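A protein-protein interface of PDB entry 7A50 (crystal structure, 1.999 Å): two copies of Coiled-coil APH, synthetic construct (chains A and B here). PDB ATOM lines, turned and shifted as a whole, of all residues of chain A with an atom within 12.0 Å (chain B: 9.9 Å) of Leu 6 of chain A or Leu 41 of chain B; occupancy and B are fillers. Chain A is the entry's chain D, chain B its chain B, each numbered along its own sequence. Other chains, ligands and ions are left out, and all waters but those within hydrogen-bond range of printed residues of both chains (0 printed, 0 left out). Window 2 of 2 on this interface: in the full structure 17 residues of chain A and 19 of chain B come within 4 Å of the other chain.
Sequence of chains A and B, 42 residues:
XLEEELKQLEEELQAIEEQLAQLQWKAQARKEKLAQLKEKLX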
ATOM      1  C   ACE A   1      24.930  17.957 -13.115  1.00  0.00           C
ATOM      2  O   ACE A   1      24.080  18.322 -13.950  1.00  0.00           O
ATOM      3  CH3 ACE A   1      24.681  18.135 -11.622  1.00  0.00           C
ATOM      4  N   LEU A   2      26.099  17.403 -13.456  1.00  0.00           N
ATOM      5  CA  LEU A   2      26.490  17.314 -14.861  1.00  0.00           C
ATOM      6  C   LEU A   2      25.545  16.411 -15.646  1.00  0.00           C
ATOM      7  O   LEU A   2      25.213  16.712 -16.804  1.00  0.00           O
ATOM      8  CB  LEU A   2      27.941  16.850 -14.990  1.00  0.00           C
ATOM      9  CG  LEU A   2      28.945  17.827 -14.355  1.00  0.00           C
ATOM     10  CD1 LEU A   2      30.395  17.336 -14.440  1.00  0.00           C
ATOM     11  CD2 LEU A   2      28.810  19.203 -14.968  1.00  0.00           C
ATOM     12  N   GLU A   3      25.071  15.326 -15.025  1.00  0.00           N
ATOM     13  CA  GLU A   3      24.171  14.414 -15.723  1.00  0.00           C
ATOM     14  C   GLU A   3      22.867  15.099 -16.095  1.00  0.00           C
ATOM     15  O   GLU A   3      22.331  14.869 -17.179  1.00  0.00           O
ATOM     16  CB  GLU A   3      23.849  13.198 -14.864  1.00  0.00           C
ATOM     17  CG  GLU A   3      24.979  12.256 -14.644  1.00  0.00           C
ATOM     18  CD  GLU A   3      24.624  11.212 -13.600  1.00  0.00           C
ATOM     19  OE1 GLU A   3      23.624  11.409 -12.872  1.00  0.00           O
ATOM     20  OE2 GLU A   3      25.350  10.205 -13.495  1.00  0.00           O
ATOM     21  N   GLU A   4      22.325  15.908 -15.181  1.00  0.00           N
ATOM     22  CA  GLU A   4      21.123  16.682 -15.471  1.00  0.00           C
ATOM     23  C   GLU A   4      21.402  17.745 -16.529  1.00  0.00           C
ATOM     24  O   GLU A   4      20.552  18.014 -17.394  1.00  0.00           O
ATOM     25  CB  GLU A   4      20.588  17.297 -14.176  1.00  0.00           C
ATOM     26  CG  GLU A   4      19.215  17.935 -14.292  1.00  0.00           C
ATOM     27  CD  GLU A   4      18.113  16.949 -14.675  1.00  0.00           C
ATOM     28  OE1 GLU A   4      18.330  15.719 -14.592  1.00  0.00           O
ATOM     29  OE2 GLU A   4      17.018  17.410 -15.059  1.00  0.00           O
ATOM     30  N   GLU A   5      22.580  18.373 -16.479  1.00  0.00           N
ATOM     31  CA  GLU A   5      22.938  19.290 -17.557  1.00  0.00           C
ATOM     32  C   GLU A   5      22.915  18.566 -18.895  1.00  0.00           C
ATOM     33  O   GLU A   5      22.333  19.059 -19.871  1.00  0.00           O
ATOM     34  CB  GLU A   5      24.317  19.902 -17.315  1.00  0.00           C
ATOM     35  CG  GLU A   5      24.371  20.951 -16.229  1.00  0.00           C
ATOM     36  CD  GLU A   5      25.746  21.587 -16.121  1.00  0.00           C
ATOM     37  OE1 GLU A   5      26.269  21.710 -14.991  1.00  0.00           O
ATOM     38  OE2 GLU A   5      26.311  21.947 -17.175  1.00  0.00           O
ATOM     39  N   LEU A   6      23.488  17.362 -18.941  1.00  0.00           N
ATOM     40  CA  LEU A   6      23.488  16.593 -20.180  1.00  0.00           C
ATOM     41  C   LEU A   6      22.064  16.354 -20.664  1.00  0.00           C
ATOM     42  O   LEU A   6      21.752  16.591 -21.837  1.00  0.00           O
ATOM     43  CB  LEU A   6      24.221  15.268 -19.988  1.00  0.00           C
ATOM     44  CG  LEU A   6      24.476  14.408 -21.231  1.00  0.00           C
ATOM     45  CD1 LEU A   6      25.728  13.570 -21.018  1.00  0.00           C
ATOM     46  CD2 LEU A   6      23.318  13.481 -21.505  1.00  0.00           C
ATOM     47  N   LYS A   7      21.192  15.883 -19.757  1.00  0.00           N
ATOM     48  CA  LYS A   7      19.800  15.590 -20.094  1.00  0.00           C
ATOM     49  C   LYS A   7      19.086  16.818 -20.646  1.00  0.00           C
ATOM     50  O   LYS A   7      18.374  16.738 -21.657  1.00  0.00           O
ATOM     51  CB  LYS A   7      19.075  15.069 -18.851  1.00  0.00           C
ATOM     52  CG  LYS A   7      17.559  15.101 -18.949  1.00  0.00           C
ATOM     53  CD  LYS A   7      16.910  14.781 -17.597  1.00  0.00           C
ATOM     54  CE  LYS A   7      15.504  15.376 -17.476  1.00  0.00           C
ATOM     55  NZ  LYS A   7      14.854  15.023 -16.176  1.00  0.00           N
ATOM     56  N   GLN A   8      19.272  17.965 -19.993  1.00  0.00           N
ATOM     57  CA  GLN A   8      18.599  19.188 -20.410  1.00  0.00           C
ATOM     58  C   GLN A   8      19.134  19.667 -21.751  1.00  0.00           C
ATOM     59  O   GLN A   8      18.378  20.173 -22.592  1.00  0.00           O
ATOM     60  CB  GLN A   8      18.783  20.255 -19.332  1.00  0.00           C
ATOM     61  CG  GLN A   8      18.007  19.951 -18.051  1.00  0.00           C
ATOM     62  CD  GLN A   8      18.317  20.923 -16.921  1.00  0.00           C
ATOM     63  OE1 GLN A   8      18.113  20.610 -15.744  1.00  0.00           O
ATOM     64  NE2 GLN A   8      18.822  22.103 -17.274  1.00  0.00           N
ATOM     65  N   LEU A   9      20.442  19.537 -21.956  1.00  0.00           N
ATOM     66  CA  LEU A   9      21.024  19.832 -23.259  1.00  0.00           C
ATOM     67  C   LEU A   9      20.406  18.954 -24.349  1.00  0.00           C
ATOM     68  O   LEU A   9      20.057  19.440 -25.431  1.00  0.00           O
ATOM     69  CB  LEU A   9      22.532  19.649 -23.181  1.00  0.00           C
ATOM     70  CG  LEU A   9      23.402  19.726 -24.416  1.00  0.00           C
ATOM     71  CD1 LEU A   9      23.164  21.057 -25.115  1.00  0.00           C
ATOM     72  CD2 LEU A   9      24.849  19.606 -23.977  1.00  0.00           C
ATOM     73  N   GLU A  10      20.265  17.650 -24.071  1.00  0.00           N
ATOM     74  CA  GLU A  10      19.678  16.724 -25.038  1.00  0.00           C
ATOM     75  C   GLU A  10      18.212  17.035 -25.300  1.00  0.00           C
ATOM     76  O   GLU A  10      17.748  16.933 -26.443  1.00  0.00           O
ATOM     77  CB  GLU A  10      19.841  15.276 -24.557  1.00  0.00           C
ATOM     78  CG  GLU A  10      21.255  14.750 -24.726  1.00  0.00           C
ATOM     79  CD  GLU A  10      21.419  13.318 -24.231  1.00  0.00           C
ATOM     80  OE1 GLU A  10      22.090  12.531 -24.931  1.00  0.00           O
ATOM     81  OE2 GLU A  10      20.847  12.980 -23.169  1.00  0.00           O
ATOM     82  N   GLU A  11      17.466  17.436 -24.270  1.00  0.00           N
ATOM     83  CA  GLU A  11      16.084  17.862 -24.495  1.00  0.00           C
ATOM     84  C   GLU A  11      16.030  19.129 -25.336  1.00  0.00           C
ATOM     85  O   GLU A  11      15.168  19.263 -26.213  1.00  0.00           O
ATOM     86  CB  GLU A  11      15.377  18.048 -23.151  1.00  0.00           C
ATOM     87  CG  GLU A  11      15.242  16.697 -22.396  1.00  0.00           C
ATOM     88  CD  GLU A  11      14.733  16.813 -20.961  1.00  0.00           C
ATOM     89  OE1 GLU A  11      14.476  15.750 -20.342  1.00  0.00           O
ATOM     90  OE2 GLU A  11      14.570  17.948 -20.462  1.00  0.00           O
ATOM     91  N   GLU A  12      16.936  20.082 -25.091  1.00  0.00           N
ATOM     92  CA  GLU A  12      16.902  21.299 -25.895  1.00  0.00           C
ATOM     93  C   GLU A  12      17.197  20.981 -27.353  1.00  0.00           C
ATOM     94  O   GLU A  12      16.522  21.485 -28.266  1.00  0.00           O
ATOM     95  CB  GLU A  12      17.886  22.332 -25.351  1.00  0.00           C
ATOM     96  CG  GLU A  12      17.431  22.924 -24.030  1.00  0.00           C
ATOM     97  CD  GLU A  12      18.293  24.088 -23.575  1.00  0.00           C
ATOM     98  OE1 GLU A  12      19.415  24.244 -24.102  1.00  0.00           O
ATOM     99  OE2 GLU A  12      17.837  24.853 -22.695  1.00  0.00           O
ATOM    100  N   LEU A  13      18.195  20.125 -27.584  1.00  0.00           N
ATOM    101  CA  LEU A  13      18.527  19.704 -28.936  1.00  0.00           C
ATOM    102  C   LEU A  13      17.333  19.040 -29.617  1.00  0.00           C
ATOM    103  O   LEU A  13      17.048  19.317 -30.786  1.00  0.00           O
ATOM    104  CB  LEU A  13      19.723  18.763 -28.878  1.00  0.00           C
ATOM    105  CG  LEU A  13      20.857  18.810 -29.893  1.00  0.00           C
ATOM    106  CD1 LEU A  13      21.167  20.234 -30.348  1.00  0.00           C
ATOM    107  CD2 LEU A  13      22.097  18.162 -29.268  1.00  0.00           C
ATOM    108  N   GLN A  14      16.596  18.188 -28.892  1.00  0.00           N
ATOM    109  CA  GLN A  14      15.414  17.563 -29.493  1.00  0.00           C
ATOM    110  C   GLN A  14      14.342  18.600 -29.797  1.00  0.00           C
ATOM    111  O   GLN A  14      13.712  18.555 -30.856  1.00  0.00           O
ATOM    112  CB  GLN A  14      14.857  16.467 -28.578  1.00  0.00           C
ATOM    113  CG  GLN A  14      13.760  15.672 -29.270  1.00  0.00           C
ATOM    114  CD  GLN A  14      14.261  15.037 -30.567  1.00  0.00           C
ATOM    115  OE1 GLN A  14      15.204  14.243 -30.548  1.00  0.00           O
ATOM    116  NE2 GLN A  14      13.641  15.400 -31.700  1.00  0.00           N
ATOM    117  N   ALA A  15      14.139  19.555 -28.884  1.00  0.00           N
ATOM    118  CA  ALA A  15      13.171  20.619 -29.122  1.00  0.00           C
ATOM    119  C   ALA A  15      13.547  21.454 -30.348  1.00  0.00           C
ATOM    120  O   ALA A  15      12.666  21.895 -31.099  1.00  0.00           O
ATOM    121  CB  ALA A  15      13.044  21.493 -27.875  1.00  0.00           C
ATOM    122  N   ILE A  16      14.849  21.705 -30.558  1.00  0.00           N
ATOM    123  CA  ILE A  16      15.273  22.435 -31.755  1.00  0.00           C
ATOM    124  C   ILE A  16      15.047  21.593 -33.013  1.00  0.00           C
ATOM    125  O   ILE A  16      14.625  22.112 -34.057  1.00  0.00           O
ATOM    126  CB  ILE A  16      16.735  22.896 -31.629  1.00  0.00           C
ATOM    127  CG1 ILE A  16      16.863  23.924 -30.498  1.00  0.00           C
ATOM    128  CG2 ILE A  16      17.188  23.505 -32.958  1.00  0.00           C
ATOM    129  CD1 ILE A  16      18.336  24.175 -29.976  1.00  0.00           C
ATOM    130  N   ARG B  30      24.895  23.761 -29.332  1.00  0.00           N
ATOM    131  CA  ARG B  30      24.580  22.750 -28.333  1.00  0.00           C
ATOM    132  C   ARG B  30      25.241  21.409 -28.655  1.00  0.00           C
ATOM    133  O   ARG B  30      25.615  20.672 -27.733  1.00  0.00           O
ATOM    134  CB  ARG B  30      23.059  22.616 -28.199  1.00  0.00           C
ATOM    135  CG  ARG B  30      22.442  23.707 -27.281  1.00  0.00           C
ATOM    136  CD  ARG B  30      20.915  23.948 -27.559  1.00  0.00           C
ATOM    137  NE  ARG B  30      20.405  24.963 -26.637  1.00  0.00           N
ATOM    138  CZ  ARG B  30      20.538  26.269 -26.834  1.00  0.00           C
ATOM    139  NH1 ARG B  30      21.101  26.705 -27.954  1.00  0.00           N
ATOM    140  NH2 ARG B  30      20.094  27.130 -25.930  1.00  0.00           N
ATOM    141  N   LYS B  33      28.786  21.700 -27.407  1.00  0.00           N
ATOM    142  CA  LYS B  33      28.828  21.571 -26.002  1.00  0.00           C
ATOM    143  C   LYS B  33      28.583  20.144 -25.589  1.00  0.00           C
ATOM    144  O   LYS B  33      29.175  19.680 -24.690  1.00  0.00           O
ATOM    145  CB  LYS B  33      27.824  22.462 -25.370  1.00  0.00           C
ATOM    146  CG  LYS B  33      27.893  22.550 -23.865  1.00  0.00           C
ATOM    147  CD  LYS B  33      29.162  23.224 -23.384  1.00  0.00           C
ATOM    148  CE  LYS B  33      29.311  23.147 -21.871  1.00  0.00           C
ATOM    149  NZ  LYS B  33      30.710  23.117 -21.339  1.00  0.00           N
ATOM    150  N   LEU B  34      27.673  19.474 -26.236  1.00  0.00           N
ATOM    151  CA  LEU B  34      27.388  18.126 -25.957  1.00  0.00           C
ATOM    152  C   LEU B  34      28.579  17.228 -26.132  1.00  0.00           C
ATOM    153  O   LEU B  34      28.804  16.393 -25.346  1.00  0.00           O
ATOM    154  CB  LEU B  34      26.322  17.660 -26.860  1.00  0.00           C
ATOM    155  CG  LEU B  34      25.806  16.353 -26.446  1.00  0.00           C
ATOM    156  CD1 LEU B  34      24.964  16.636 -25.264  1.00  0.00           C
ATOM    157  CD2 LEU B  34      24.976  15.798 -27.557  1.00  0.00           C
ATOM    158  N   ALA B  35      29.303  17.361 -27.209  1.00  0.00           N
ATOM    159  CA  ALA B  35      30.481  16.522 -27.394  1.00  0.00           C
ATOM    160  C   ALA B  35      31.503  16.768 -26.287  1.00  0.00           C
ATOM    161  O   ALA B  35      32.106  15.816 -25.766  1.00  0.00           O
ATOM    162  CB  ALA B  35      31.101  16.770 -28.763  1.00  0.00           C
ATOM    163  N   GLN B  36      31.703  18.039 -25.909  1.00  0.00           N
ATOM    164  CA  GLN B  36      32.611  18.370 -24.815  1.00  0.00           C
ATOM    165  C   GLN B  36      32.138  17.739 -23.513  1.00  0.00           C
ATOM    166  O   GLN B  36      32.938  17.177 -22.758  1.00  0.00           O
ATOM    167  CB  GLN B  36      32.720  19.882 -24.648  1.00  0.00           C
ATOM    168  CG  GLN B  36      33.272  20.620 -25.857  1.00  0.00           C
ATOM    169  CD  GLN B  36      33.210  22.129 -25.679  1.00  0.00           C
ATOM    170  OE1 GLN B  36      32.921  22.621 -24.587  1.00  0.00           O
ATOM    171  NE2 GLN B  36      33.442  22.867 -26.761  1.00  0.00           N
ATOM    172  N   LEU B  37      30.836  17.843 -23.222  1.00  0.00           N
ATOM    173  CA  LEU B  37      30.319  17.247 -21.998  1.00  0.00           C
ATOM    174  C   LEU B  37      30.494  15.733 -22.008  1.00  0.00           C
ATOM    175  O   LEU B  37      30.920  15.145 -21.002  1.00  0.00           O
ATOM    176  CB  LEU B  37      28.860  17.629 -21.802  1.00  0.00           C
ATOM    177  CG  LEU B  37      28.337  17.361 -20.394  1.00  0.00           C
ATOM    178  CD1 LEU B  37      29.144  18.093 -19.332  1.00  0.00           C
ATOM    179  CD2 LEU B  37      26.882  17.756 -20.333  1.00  0.00           C
ATOM    180  N   LYS B  38      30.216  15.093 -23.147  1.00  0.00           N
ATOM    181  CA  LYS B  38      30.412  13.651 -23.242  1.00  0.00           C
ATOM    182  C   LYS B  38      31.877  13.278 -23.043  1.00  0.00           C
ATOM    183  O   LYS B  38      32.179  12.247 -22.437  1.00  0.00           O
ATOM    184  CB  LYS B  38      29.921  13.133 -24.590  1.00  0.00           C
ATOM    185  CG  LYS B  38      28.420  13.092 -24.748  1.00  0.00           C
ATOM    186  CD  LYS B  38      28.067  12.371 -26.041  1.00  0.00           C
ATOM    187  CE  LYS B  38      26.573  12.355 -26.277  1.00  0.00           C
ATOM    188  NZ  LYS B  38      26.270  11.866 -27.644  1.00  0.00           N
ATOM    189  N   GLU B  39      32.802  14.107 -23.544  1.00  0.00           N
ATOM    190  CA  GLU B  39      34.219  13.842 -23.302  1.00  0.00           C
ATOM    191  C   GLU B  39      34.577  13.990 -21.824  1.00  0.00           C
ATOM    192  O   GLU B  39      35.324  13.169 -21.289  1.00  0.00           O
ATOM    193  CB  GLU B  39      35.099  14.748 -24.164  1.00  0.00           C
ATOM    194  CG  GLU B  39      36.577  14.358 -24.083  1.00  0.00           C
ATOM    195  CD  GLU B  39      37.491  15.264 -24.891  1.00  0.00           C
ATOM    196  OE1 GLU B  39      38.660  14.866 -25.116  1.00  0.00           O
ATOM    197  OE2 GLU B  39      37.055  16.375 -25.271  1.00  0.00           O
ATOM    198  N   LYS B  40      34.051  15.022 -21.150  1.00  0.00           N
ATOM    199  CA  LYS B  40      34.268  15.170 -19.710  1.00  0.00           C
ATOM    200  C   LYS B  40      33.762  13.956 -18.939  1.00  0.00           C
ATOM    201  O   LYS B  40      34.422  13.473 -18.002  1.00  0.00           O
ATOM    202  CB  LYS B  40      33.553  16.420 -19.192  1.00  0.00           C
ATOM    203  CG  LYS B  40      34.006  16.876 -17.803  1.00  0.00           C
ATOM    204  CD  LYS B  40      33.323  18.184 -17.403  1.00  0.00           C
ATOM    205  CE  LYS B  40      33.542  19.286 -18.423  1.00  0.00           C
ATOM    206  NZ  LYS B  40      32.677  20.485 -18.172  1.00  0.00           N
ATOM    207  N   LEU B  41      32.587  13.464 -19.306  1.00  0.00           N
ATOM    208  CA  LEU B  41      31.963  12.353 -18.611  1.00  0.00           C
ATOM    209  C   LEU B  41      32.585  11.024 -19.025  1.00  0.00           C
ATOM    210  O   LEU B  41      32.495  10.052 -18.285  1.00  0.00           O
ATOM    211  CB  LEU B  41      30.449  12.339 -18.861  1.00  0.00           C
ATOM    212  CG  LEU B  41      29.722  13.553 -18.273  1.00  0.00           C
ATOM    213  CD1 LEU B  41      28.274  13.559 -18.693  1.00  0.00           C
ATOM    214  CD2 LEU B  41      29.816  13.510 -16.781  1.00  0.00           C
ATOM    215  N   NH2 B  42      33.216  10.995 -20.199  1.00  0.00           N
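The guanidinium group (NE) of Arg 30 of chain B is in salt-bridge range of the side-chain carboxylate (OE1) of Glu 12 of chain A (2.8 Å).
Among the printed residues, merely in contact across the chains: Leu 9 of chain A with Leu 34 of chain B, Leu 6 of chain A with Leu 41 of chain B, Leu 9 of chain A with Arg 30 of chain B, Ile 16 of chain A with Arg 30 of chain B, Leu 6 of chain A with Leu 37 of chain B and Leu 13 of chain A with Arg 30 of chain B.
No position is printed for both chains.
Of the printed residues of chain B, Leu 6 of chain A touches Leu 37 and Leu 41. Of chain B, only Arg 30 and Leu 34 come within 4 Å of Leu 9 of chain A. Of chain A, only Leu 9 (3.2 Å) comes within 4 Å of Leu 34 of chain B. Leu 37 of chain B touches just one residue of chain A: Leu 6 (3.6 Å). No residue of chain A comes within 4 Å of Lys 38 of chain B. Of the printed residues of chain B, Glu 12 of chain A touches Arg 30. Of the printed residues of chain A, Arg 30 of chain B touches Leu 9 (3.5 Å), Glu 12 (2.8 Å), Leu 13 (3.7 Å) and Ile 16 (3.5 Å). Printed residues of chain B within 4 Å of Ile 16 of chain A: Arg 30. Printed residues of chain B within 4 Å of Leu 13 of chain A: Arg 30. Gln 8 of chain A touches none of the printed residues of chain B.
Hydrophobic or aromatic side chains of chain A within 4 Å of the printed part of chain B: Leu 6, Leu 9, Leu 13 and Ile 16. Of the 11 printed residues of chain B, 4 touch a printed residue of chain A. Hydrophobic or aromatic side chains of chain B within 4 Å of the printed part of chain A: Leu 34, Leu 37 and Leu 41. Among the printed residues, 7 pairs touch across the chains. Among the printed residues, Asp or Glu carboxylates within 4 Å of a Lys or Arg side-chain nitrogen of the other chain: Glu 12 of chain A with Arg 30 of chain B (2.8 Å).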
